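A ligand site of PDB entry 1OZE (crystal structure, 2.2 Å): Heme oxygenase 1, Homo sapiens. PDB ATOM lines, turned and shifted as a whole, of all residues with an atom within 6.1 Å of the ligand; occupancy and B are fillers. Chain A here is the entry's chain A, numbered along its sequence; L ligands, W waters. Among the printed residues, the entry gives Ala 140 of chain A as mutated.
Merely in contact with the ligand: Asn 210 (3.1 Å), Thr 135 (3.3 Å), Ser 142 (3.3 Å), Gly 139 (3.3 Å), Glu 29 (3.4 Å), Arg 136 (3.4 Å), Gly 143 (3.5 Å), Phe 207 (3.6 Å), Met 34 (3.6 Å), Gln 38 (3.8 Å), Leu 138 (3.8 Å), Ala 28 (3.8 Å) and Leu 147 (3.97 Å). Of the 29 residues printed, 17 come within 4 Å of the ligand.
OH of Tyr 134 lies within hydrogen-bond range of N of Lys 18 (3.4 Å). O of Lys 18 sits at hydrogen-bond distance from OG1 of Thr 21. The side-chain amide oxygen (OD1) of Asn 210 is in hydrogen-bond range of the guanidinium group (NH1) of Arg 136, at 3.1 Å. OH of Tyr 114 sits at hydrogen-bond distance from ND2 of Asn 210, at 3.1 Å. The side-chain hydroxyl (OG) of Ser 142 sits at hydrogen-bond distance from the backbone carbonyl oxygen (O) of Leu 138, at 3.0 Å. NE2 of Gln 38 sits at hydrogen-bond distance from O of Glu 29, at 2.7 Å. The guanidinium group (NH1) of Arg 136 lies within hydrogen-bond range of the side-chain hydroxyl (OH) of Tyr 114, 3.0 Å away. The side-chain amide nitrogen (NE2) of Gln 38 sits at hydrogen-bond distance from the backbone carbonyl oxygen (O) of Met 34, 3.0 Å away.
Water W2 lies within hydrogen-bond range of O3 of the ligand, O of Ser 14 and NE of Arg 183.
FE1 of the ligand is bound by NE2 of His 25. OH of Tyr 134 is in hydrogen-bond range of O3 of the ligand (2.4 Å). The guanidinium group (NH2) of Arg 183 is in salt-bridge range of an oxygen (O4) of the ligand (2.9 Å). The side-chain amino group (NZ) of Lys 18 is in salt-bridge range of an oxygen (O1) of the ligand.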
ATOM      1  N   SER A  14     -20.710  29.501   3.296  1.00  0.00           N
ATOM      2  CA  SER A  14     -21.094  28.271   3.986  1.00  0.00           C
ATOM      3  C   SER A  14     -22.594  28.035   3.846  1.00  0.00           C
ATOM      4  O   SER A  14     -23.065  26.901   3.806  1.00  0.00           O
ATOM      5  CB  SER A  14     -20.708  28.330   5.472  1.00  0.00           C
ATOM      6  OG  SER A  14     -21.424  29.347   6.147  1.00  0.00           O
ATOM      7  N   LEU A  17     -23.177  27.087   0.032  1.00  0.00           N
ATOM      8  CA  LEU A  17     -22.768  25.720  -0.232  1.00  0.00           C
ATOM      9  C   LEU A  17     -23.821  24.708   0.203  1.00  0.00           C
ATOM     10  O   LEU A  17     -24.249  23.874  -0.581  1.00  0.00           O
ATOM     11  CB  LEU A  17     -21.441  25.423   0.476  1.00  0.00           C
ATOM     12  CG  LEU A  17     -20.185  26.052  -0.139  1.00  0.00           C
ATOM     13  CD1 LEU A  17     -19.003  25.764   0.749  1.00  0.00           C
ATOM     14  CD2 LEU A  17     -19.952  25.497  -1.542  1.00  0.00           C
ATOM     15  N   LYS A  18     -24.250  24.794   1.458  1.00  0.00           N
ATOM     16  CA  LYS A  18     -25.256  23.885   1.957  1.00  0.00           C
ATOM     17  C   LYS A  18     -26.507  23.933   1.086  1.00  0.00           C
ATOM     18  O   LYS A  18     -27.059  22.885   0.729  1.00  0.00           O
ATOM     19  CB  LYS A  18     -25.611  24.244   3.401  1.00  0.00           C
ATOM     20  CG  LYS A  18     -26.643  23.315   4.011  1.00  0.00           C
ATOM     21  CD  LYS A  18     -26.859  23.569   5.491  1.00  0.00           C
ATOM     22  CE  LYS A  18     -27.838  22.559   6.078  1.00  0.00           C
ATOM     23  NZ  LYS A  18     -28.052  22.765   7.539  1.00  0.00           N
ATOM     24  N   GLU A  19     -26.941  25.140   0.745  1.00  0.00           N
ATOM     25  CA  GLU A  19     -28.128  25.355  -0.065  1.00  0.00           C
ATOM     26  C   GLU A  19     -28.050  24.744  -1.461  1.00  0.00           C
ATOM     27  O   GLU A  19     -28.964  24.052  -1.900  1.00  0.00           O
ATOM     28  CB  GLU A  19     -28.415  26.854  -0.190  1.00  0.00           C
ATOM     29  CG  GLU A  19     -29.607  27.217  -1.065  1.00  0.00           C
ATOM     30  N   THR A  21     -26.077  22.344  -2.530  1.00  0.00           N
ATOM     31  CA  THR A  21     -25.789  20.909  -2.587  1.00  0.00           C
ATOM     32  C   THR A  21     -26.858  20.001  -2.006  1.00  0.00           C
ATOM     33  O   THR A  21     -26.683  18.787  -1.979  1.00  0.00           O
ATOM     34  CB  THR A  21     -24.438  20.577  -1.896  1.00  0.00           C
ATOM     35  OG1 THR A  21     -24.489  20.974  -0.518  1.00  0.00           O
ATOM     36  CG2 THR A  21     -23.296  21.282  -2.600  1.00  0.00           C
ATOM     37  N   HIS A  25     -26.869  16.089  -2.643  1.00  0.00           N
ATOM     38  CA  HIS A  25     -26.662  15.313  -1.415  1.00  0.00           C
ATOM     39  C   HIS A  25     -27.758  14.250  -1.353  1.00  0.00           C
ATOM     40  O   HIS A  25     -27.504  13.108  -0.970  1.00  0.00           O
ATOM     41  CB  HIS A  25     -26.730  16.221  -0.177  1.00  0.00           C
ATOM     42  CG  HIS A  25     -26.374  15.521   1.105  1.00  0.00           C
ATOM     43  ND1 HIS A  25     -27.212  14.615   1.717  1.00  0.00           N
ATOM     44  CD2 HIS A  25     -25.254  15.579   1.873  1.00  0.00           C
ATOM     45  CE1 HIS A  25     -26.634  14.156   2.808  1.00  0.00           C
ATOM     46  NE2 HIS A  25     -25.449  14.722   2.926  1.00  0.00           N
ATOM     47  N   ALA A  28     -26.989  11.427  -3.509  1.00  0.00           N
ATOM     48  CA  ALA A  28     -25.996  10.569  -2.892  1.00  0.00           C
ATOM     49  C   ALA A  28     -26.727   9.568  -2.000  1.00  0.00           C
ATOM     50  O   ALA A  28     -26.495   8.365  -2.090  1.00  0.00           O
ATOM     51  CB  ALA A  28     -25.017  11.398  -2.059  1.00  0.00           C
ATOM     52  N   GLU A  29     -27.631  10.067  -1.167  1.00  0.00           N
ATOM     53  CA  GLU A  29     -28.388   9.211  -0.268  1.00  0.00           C
ATOM     54  C   GLU A  29     -29.241   8.213  -1.032  1.00  0.00           C
ATOM     55  O   GLU A  29     -29.438   7.085  -0.579  1.00  0.00           O
ATOM     56  CB  GLU A  29     -29.285  10.063   0.628  1.00  0.00           C
ATOM     57  CG  GLU A  29     -28.562  11.183   1.327  1.00  0.00           C
ATOM     58  CD  GLU A  29     -29.493  12.048   2.153  1.00  0.00           C
ATOM     59  OE1 GLU A  29     -30.030  11.537   3.155  1.00  0.00           O
ATOM     60  OE2 GLU A  29     -29.693  13.232   1.795  1.00  0.00           O
ATOM     61  N   ASN A  30     -29.731   8.616  -2.207  1.00  0.00           N
ATOM     62  CA  ASN A  30     -30.575   7.752  -3.025  1.00  0.00           C
ATOM     63  C   ASN A  30     -29.802   6.693  -3.823  1.00  0.00           C
ATOM     64  O   ASN A  30     -30.402   5.736  -4.314  1.00  0.00           O
ATOM     65  CB  ASN A  30     -31.417   8.580  -3.990  1.00  0.00           C
ATOM     66  CG  ASN A  30     -32.487   9.395  -3.283  1.00  0.00           C
ATOM     67  OD1 ASN A  30     -32.862   9.099  -2.154  1.00  0.00           O
ATOM     68  ND2 ASN A  30     -32.976  10.432  -3.946  1.00  0.00           N
ATOM     69  N   MET A  34     -25.672   3.288  -1.420  1.00  0.00           N
ATOM     70  CA  MET A  34     -25.910   3.983  -0.154  1.00  0.00           C
ATOM     71  C   MET A  34     -27.278   3.651   0.413  1.00  0.00           C
ATOM     72  O   MET A  34     -27.499   3.752   1.616  1.00  0.00           O
ATOM     73  CB  MET A  34     -25.754   5.493  -0.333  1.00  0.00           C
ATOM     74  CG  MET A  34     -24.309   5.959  -0.335  1.00  0.00           C
ATOM     75  SD  MET A  34     -23.468   5.654   1.251  1.00  0.00           S
ATOM     76  CE  MET A  34     -22.718   4.099   0.969  1.00  0.00           C
ATOM     77  N   GLN A  38     -27.679   2.416   4.143  1.00  0.00           N
ATOM     78  CA  GLN A  38     -28.586   3.000   5.124  1.00  0.00           C
ATOM     79  C   GLN A  38     -29.606   1.989   5.657  1.00  0.00           C
ATOM     80  O   GLN A  38     -30.065   2.101   6.795  1.00  0.00           O
ATOM     81  CB  GLN A  38     -29.306   4.210   4.506  1.00  0.00           C
ATOM     82  CG  GLN A  38     -28.357   5.302   4.054  1.00  0.00           C
ATOM     83  CD  GLN A  38     -29.056   6.386   3.252  1.00  0.00           C
ATOM     84  OE1 GLN A  38     -29.833   7.160   3.791  1.00  0.00           O
ATOM     85  NE2 GLN A  38     -28.781   6.420   1.950  1.00  0.00           N
ATOM     86  N   TYR A 114     -11.883  10.433  -9.318  1.00  0.00           N
ATOM     87  CA  TYR A 114     -12.055  11.345  -8.202  1.00  0.00           C
ATOM     88  C   TYR A 114     -10.682  11.929  -7.862  1.00  0.00           C
ATOM     89  O   TYR A 114     -10.516  13.154  -7.751  1.00  0.00           O
ATOM     90  CB  TYR A 114     -12.618  10.597  -6.990  1.00  0.00           C
ATOM     91  CG  TYR A 114     -13.346  11.456  -5.971  1.00  0.00           C
ATOM     92  CD1 TYR A 114     -12.933  12.763  -5.696  1.00  0.00           C
ATOM     93  CD2 TYR A 114     -14.406  10.930  -5.238  1.00  0.00           C
ATOM     94  CE1 TYR A 114     -13.563  13.519  -4.717  1.00  0.00           C
ATOM     95  CE2 TYR A 114     -15.039  11.662  -4.261  1.00  0.00           C
ATOM     96  CZ  TYR A 114     -14.621  12.961  -3.996  1.00  0.00           C
ATOM     97  OH  TYR A 114     -15.247  13.664  -2.991  1.00  0.00           O
ATOM     98  N   TYR A 134     -14.447  21.125   2.128  1.00  0.00           N
ATOM     99  CA  TYR A 134     -15.749  21.312   2.757  1.00  0.00           C
ATOM    100  C   TYR A 134     -16.568  20.036   2.642  1.00  0.00           C
ATOM    101  O   TYR A 134     -17.094  19.509   3.625  1.00  0.00           O
ATOM    102  CB  TYR A 134     -16.480  22.461   2.052  1.00  0.00           C
ATOM    103  CG  TYR A 134     -17.977  22.463   2.230  1.00  0.00           C
ATOM    104  CD1 TYR A 134     -18.558  22.856   3.436  1.00  0.00           C
ATOM    105  CD2 TYR A 134     -18.812  22.052   1.185  1.00  0.00           C
ATOM    106  CE1 TYR A 134     -19.961  22.841   3.591  1.00  0.00           C
ATOM    107  CE2 TYR A 134     -20.202  22.039   1.336  1.00  0.00           C
ATOM    108  CZ  TYR A 134     -20.770  22.435   2.537  1.00  0.00           C
ATOM    109  OH  TYR A 134     -22.143  22.414   2.665  1.00  0.00           O
ATOM    110  N   THR A 135     -16.692  19.552   1.416  1.00  0.00           N
ATOM    111  CA  THR A 135     -17.446  18.345   1.132  1.00  0.00           C
ATOM    112  C   THR A 135     -16.926  17.118   1.910  1.00  0.00           C
ATOM    113  O   THR A 135     -17.728  16.385   2.481  1.00  0.00           O
ATOM    114  CB  THR A 135     -17.446  18.075  -0.390  1.00  0.00           C
ATOM    115  OG1 THR A 135     -18.342  18.994  -1.020  1.00  0.00           O
ATOM    116  CG2 THR A 135     -17.890  16.669  -0.702  1.00  0.00           C
ATOM    117  N   ARG A 136     -15.620  16.901   1.939  1.00  0.00           N
ATOM    118  CA  ARG A 136     -15.093  15.750   2.648  1.00  0.00           C
ATOM    119  C   ARG A 136     -15.128  15.910   4.158  1.00  0.00           C
ATOM    120  O   ARG A 136     -15.730  15.099   4.870  1.00  0.00           O
ATOM    121  CB  ARG A 136     -13.646  15.459   2.247  1.00  0.00           C
ATOM    122  CG  ARG A 136     -13.396  15.143   0.788  1.00  0.00           C
ATOM    123  CD  ARG A 136     -14.418  14.176   0.192  1.00  0.00           C
ATOM    124  NE  ARG A 136     -14.713  13.009   1.022  1.00  0.00           N
ATOM    125  CZ  ARG A 136     -15.407  11.952   0.599  1.00  0.00           C
ATOM    126  NH1 ARG A 136     -15.856  11.929  -0.653  1.00  0.00           N
ATOM    127  NH2 ARG A 136     -15.683  10.946   1.417  1.00  0.00           N
ATOM    128  N   LEU A 138     -16.410  18.551   6.289  1.00  0.00           N
ATOM    129  CA  LEU A 138     -17.627  18.955   6.979  1.00  0.00           C
ATOM    130  C   LEU A 138     -18.660  17.830   6.858  1.00  0.00           C
ATOM    131  O   LEU A 138     -19.438  17.586   7.772  1.00  0.00           O
ATOM    132  CB  LEU A 138     -18.170  20.266   6.399  1.00  0.00           C
ATOM    133  CG  LEU A 138     -18.773  21.200   7.468  1.00  0.00           C
ATOM    134  CD1 LEU A 138     -17.692  21.535   8.477  1.00  0.00           C
ATOM    135  CD2 LEU A 138     -19.299  22.473   6.830  1.00  0.00           C
ATOM    136  N   GLY A 139     -18.656  17.144   5.711  1.00  0.00           N
ATOM    137  CA  GLY A 139     -19.576  16.036   5.531  1.00  0.00           C
ATOM    138  C   GLY A 139     -19.289  14.901   6.499  1.00  0.00           C
ATOM    139  O   GLY A 139     -20.187  14.427   7.202  1.00  0.00           O
ATOM    140  N   ALA A 140     -18.033  14.473   6.552  1.00  0.00           N
ATOM    141  CA  ALA A 140     -17.608  13.400   7.429  1.00  0.00           C
ATOM    142  C   ALA A 140     -17.888  13.724   8.894  1.00  0.00           C
ATOM    143  O   ALA A 140     -18.194  12.840   9.695  1.00  0.00           O
ATOM    144  CB  ALA A 140     -16.122  13.139   7.247  1.00  0.00           C
ATOM    145  N   SER A 142     -20.389  15.600   9.969  1.00  0.00           N
ATOM    146  CA  SER A 142     -21.820  15.675  10.225  1.00  0.00           C
ATOM    147  C   SER A 142     -22.517  14.329  10.118  1.00  0.00           C
ATOM    148  O   SER A 142     -23.055  13.821  11.098  1.00  0.00           O
ATOM    149  CB  SER A 142     -22.472  16.667   9.264  1.00  0.00           C
ATOM    150  OG  SER A 142     -21.913  17.961   9.405  1.00  0.00           O
ATOM    151  N   GLY A 143     -22.510  13.746   8.929  1.00  0.00           N
ATOM    152  CA  GLY A 143     -23.161  12.463   8.746  1.00  0.00           C
ATOM    153  C   GLY A 143     -22.223  11.297   8.963  1.00  0.00           C
ATOM    154  O   GLY A 143     -22.535  10.157   8.609  1.00  0.00           O
ATOM    155  N   GLY A 144     -21.065  11.589   9.530  1.00  0.00           N
ATOM    156  CA  GLY A 144     -20.086  10.538   9.776  1.00  0.00           C
ATOM    157  C   GLY A 144     -20.525   9.576  10.855  1.00  0.00           C
ATOM    158  O   GLY A 144     -20.361   8.368  10.721  1.00  0.00           O
ATOM    159  N   VAL A 146     -23.624   8.843  11.887  1.00  0.00           N
ATOM    160  CA  VAL A 146     -24.753   8.015  11.475  1.00  0.00           C
ATOM    161  C   VAL A 146     -24.300   6.813  10.661  1.00  0.00           C
ATOM    162  O   VAL A 146     -24.813   5.698  10.821  1.00  0.00           O
ATOM    163  CB  VAL A 146     -25.822   8.822  10.657  1.00  0.00           C
ATOM    164  CG1 VAL A 146     -26.241  10.064  11.439  1.00  0.00           C
ATOM    165  CG2 VAL A 146     -25.269   9.221   9.305  1.00  0.00           C
ATOM    166  N   LEU A 147     -23.310   7.028   9.793  1.00  0.00           N
ATOM    167  CA  LEU A 147     -22.803   5.948   8.958  1.00  0.00           C
ATOM    168  C   LEU A 147     -21.930   4.970   9.754  1.00  0.00           C
ATOM    169  O   LEU A 147     -21.927   3.774   9.467  1.00  0.00           O
ATOM    170  CB  LEU A 147     -22.038   6.524   7.773  1.00  0.00           C
ATOM    171  CG  LEU A 147     -22.881   7.482   6.921  1.00  0.00           C
ATOM    172  CD1 LEU A 147     -22.042   8.003   5.764  1.00  0.00           C
ATOM    173  CD2 LEU A 147     -24.114   6.769   6.406  1.00  0.00           C
ATOM    174  N   LYS A 179     -17.275  23.096  13.637  1.00  0.00           N
ATOM    175  CA  LYS A 179     -17.959  23.392  12.388  1.00  0.00           C
ATOM    176  C   LYS A 179     -18.341  24.882  12.336  1.00  0.00           C
ATOM    177  O   LYS A 179     -18.375  25.461  11.259  1.00  0.00           O
ATOM    178  CB  LYS A 179     -19.202  22.505  12.211  1.00  0.00           C
ATOM    179  CG  LYS A 179     -18.863  21.050  11.939  1.00  0.00           C
ATOM    180  CD  LYS A 179     -19.805  20.397  10.911  1.00  0.00           C
ATOM    181  CE  LYS A 179     -21.233  20.238  11.421  1.00  0.00           C
ATOM    182  NZ  LYS A 179     -21.336  19.322  12.596  1.00  0.00           N
ATOM    183  N   ARG A 183     -16.938  27.215   9.373  1.00  0.00           N
ATOM    184  CA  ARG A 183     -17.857  27.981   8.524  1.00  0.00           C
ATOM    185  C   ARG A 183     -17.389  29.433   8.512  1.00  0.00           C
ATOM    186  O   ARG A 183     -17.375  30.079   7.477  1.00  0.00           O
ATOM    187  CB  ARG A 183     -19.281  27.897   9.065  1.00  0.00           C
ATOM    188  CG  ARG A 183     -19.932  26.535   8.928  1.00  0.00           C
ATOM    189  CD  ARG A 183     -21.414  26.619   9.217  1.00  0.00           C
ATOM    190  NE  ARG A 183     -22.096  25.361   8.917  1.00  0.00           N
ATOM    191  CZ  ARG A 183     -22.099  24.301   9.706  1.00  0.00           C
ATOM    192  NH1 ARG A 183     -21.445  24.322  10.867  1.00  0.00           N
ATOM    193  NH2 ARG A 183     -22.752  23.208   9.337  1.00  0.00           N
ATOM    194  N   ALA A 206     -18.209  17.372  -6.643  1.00  0.00           N
ATOM    195  CA  ALA A 206     -17.652  16.436  -5.683  1.00  0.00           C
ATOM    196  C   ALA A 206     -18.710  15.368  -5.425  1.00  0.00           C
ATOM    197  O   ALA A 206     -18.426  14.163  -5.453  1.00  0.00           O
ATOM    198  CB  ALA A 206     -17.299  17.155  -4.388  1.00  0.00           C
ATOM    199  N   PHE A 207     -19.941  15.810  -5.175  1.00  0.00           N
ATOM    200  CA  PHE A 207     -21.029  14.865  -4.935  1.00  0.00           C
ATOM    201  C   PHE A 207     -21.187  13.914  -6.128  1.00  0.00           C
ATOM    202  O   PHE A 207     -21.334  12.698  -5.955  1.00  0.00           O
ATOM    203  CB  PHE A 207     -22.344  15.602  -4.675  1.00  0.00           C
ATOM    204  CG  PHE A 207     -22.483  16.096  -3.258  1.00  0.00           C
ATOM    205  CD1 PHE A 207     -22.051  17.367  -2.901  1.00  0.00           C
ATOM    206  CD2 PHE A 207     -23.062  15.283  -2.282  1.00  0.00           C
ATOM    207  CE1 PHE A 207     -22.178  17.819  -1.583  1.00  0.00           C
ATOM    208  CE2 PHE A 207     -23.194  15.727  -0.960  1.00  0.00           C
ATOM    209  CZ  PHE A 207     -22.760  17.003  -0.616  1.00  0.00           C
ATOM    210  N   ASN A 210     -18.758  11.164  -6.245  1.00  0.00           N
ATOM    211  CA  ASN A 210     -19.060  10.182  -5.220  1.00  0.00           C
ATOM    212  C   ASN A 210     -20.161   9.264  -5.732  1.00  0.00           C
ATOM    213  O   ASN A 210     -20.125   8.049  -5.513  1.00  0.00           O
ATOM    214  CB  ASN A 210     -19.536  10.875  -3.941  1.00  0.00           C
ATOM    215  CG  ASN A 210     -18.408  11.179  -2.990  1.00  0.00           C
ATOM    216  OD1 ASN A 210     -17.843  10.283  -2.359  1.00  0.00           O
ATOM    217  ND2 ASN A 210     -18.074  12.460  -2.868  1.00  0.00           N
ATOM    218  N   PHE A 214     -20.070   5.317  -6.182  1.00  0.00           N
ATOM    219  CA  PHE A 214     -21.048   4.417  -5.575  1.00  0.00           C
ATOM    220  C   PHE A 214     -21.641   3.496  -6.643  1.00  0.00           C
ATOM    221  O   PHE A 214     -21.888   2.318  -6.387  1.00  0.00           O
ATOM    222  CB  PHE A 214     -22.200   5.205  -4.923  1.00  0.00           C
ATOM    223  CG  PHE A 214     -21.796   6.016  -3.714  1.00  0.00           C
ATOM    224  CD1 PHE A 214     -20.755   5.589  -2.873  1.00  0.00           C
ATOM    225  CD2 PHE A 214     -22.500   7.172  -3.366  1.00  0.00           C
ATOM    226  CE1 PHE A 214     -20.429   6.307  -1.722  1.00  0.00           C
ATOM    227  CE2 PHE A 214     -22.182   7.895  -2.214  1.00  0.00           C
ATOM    228  CZ  PHE A 214     -21.149   7.457  -1.379  1.00  0.00           C
HETATM  229  C1  LIG L   1     -24.211  16.777   6.238  1.00  0.00           C
HETATM  230  C2  LIG L   1     -26.005  12.265   6.248  1.00  0.00           C
HETATM  231  C3  LIG L   1     -23.358  11.196   2.340  1.00  0.00           C
HETATM  232  C4  LIG L   1     -21.435  15.674   2.422  1.00  0.00           C
HETATM  233  C5  LIG L   1     -24.874  15.602   6.612  1.00  0.00           C
HETATM  234  C6  LIG L   1     -25.681  15.440   7.823  1.00  0.00           C
HETATM  235  C7  LIG L   1     -26.241  14.228   7.745  1.00  0.00           C
HETATM  236  C8  LIG L   1     -25.728  13.576   6.572  1.00  0.00           C
HETATM  237  C9  LIG L   1     -27.190  13.629   8.783  1.00  0.00           C
HETATM  238  C10 LIG L   1     -25.738  16.244   9.122  1.00  0.00           C
HETATM  239  C11 LIG L   1     -25.736  17.765   9.277  1.00  0.00           C
HETATM  240  C12 LIG L   1     -26.975  18.422   8.694  1.00  0.00           C
HETATM  241  O1  LIG L   1     -27.236  19.599   9.038  1.00  0.00           O
HETATM  242  O2  LIG L   1     -27.668  17.773   7.886  1.00  0.00           O
HETATM  243  C13 LIG L   1     -25.461  11.612   5.165  1.00  0.00           C
HETATM  244  C14 LIG L   1     -25.832  10.269   4.813  1.00  0.00           C
HETATM  245  C15 LIG L   1     -25.121   9.954   3.698  1.00  0.00           C
HETATM  246  C16 LIG L   1     -24.288  11.126   3.375  1.00  0.00           C
HETATM  247  C17 LIG L   1     -26.925   9.408   5.463  1.00  0.00           C
HETATM  248  C18 LIG L   1     -25.240   8.730   3.042  1.00  0.00           C
HETATM  249  C19 LIG L   1     -25.688   8.579   1.656  1.00  0.00           C
HETATM  250  C20 LIG L   1     -22.581  12.318   2.026  1.00  0.00           C
HETATM  251  C21 LIG L   1     -21.654  12.393   0.915  1.00  0.00           C
HETATM  252  C22 LIG L   1     -21.084  13.621   0.986  1.00  0.00           C
HETATM  253  C23 LIG L   1     -21.685  14.328   2.112  1.00  0.00           C
HETATM  254  C24 LIG L   1     -21.438  11.368  -0.222  1.00  0.00           C
HETATM  255  C25 LIG L   1     -20.136  14.142   0.101  1.00  0.00           C
HETATM  256  C26 LIG L   1     -18.810  13.563  -0.101  1.00  0.00           C
HETATM  257  C27 LIG L   1     -22.117  16.406   3.391  1.00  0.00           C
HETATM  258  C28 LIG L   1     -21.829  17.789   3.722  1.00  0.00           C
HETATM  259  C29 LIG L   1     -22.586  18.110   4.816  1.00  0.00           C
HETATM  260  C30 LIG L   1     -23.367  16.910   5.122  1.00  0.00           C
HETATM  261  C31 LIG L   1     -20.793  18.680   3.036  1.00  0.00           C
HETATM  262  C32 LIG L   1     -22.582  19.435   5.593  1.00  0.00           C
HETATM  263  C33 LIG L   1     -23.229  20.545   4.779  1.00  0.00           C
HETATM  264  C34 LIG L   1     -23.186  21.905   5.469  1.00  0.00           C
HETATM  265  O3  LIG L   1     -23.286  22.923   4.754  1.00  0.00           O
HETATM  266  O4  LIG L   1     -23.055  21.954   6.717  1.00  0.00           O
HETATM  267  N1  LIG L   1     -24.866  14.422   5.863  1.00  0.00           N
HETATM  268  N2  LIG L   1     -24.558  12.160   4.253  1.00  0.00           N
HETATM  269  N3  LIG L   1     -22.625  13.520   2.746  1.00  0.00           N
HETATM  270  N4  LIG L   1     -23.080  15.866   4.242  1.00  0.00           N
HETATM  271 FE1  LIG L   1     -23.873  14.046   4.210  1.00  0.00          FE
HETATM  272  O   HOH W   1     -20.773  11.932   4.607  1.00  0.00           O
HETATM  273  O   HOH W   2     -22.518  25.064   5.801  1.00  0.00           O
HETATM  274  O   HOH W   3     -17.581  13.369   3.161  1.00  0.00           O
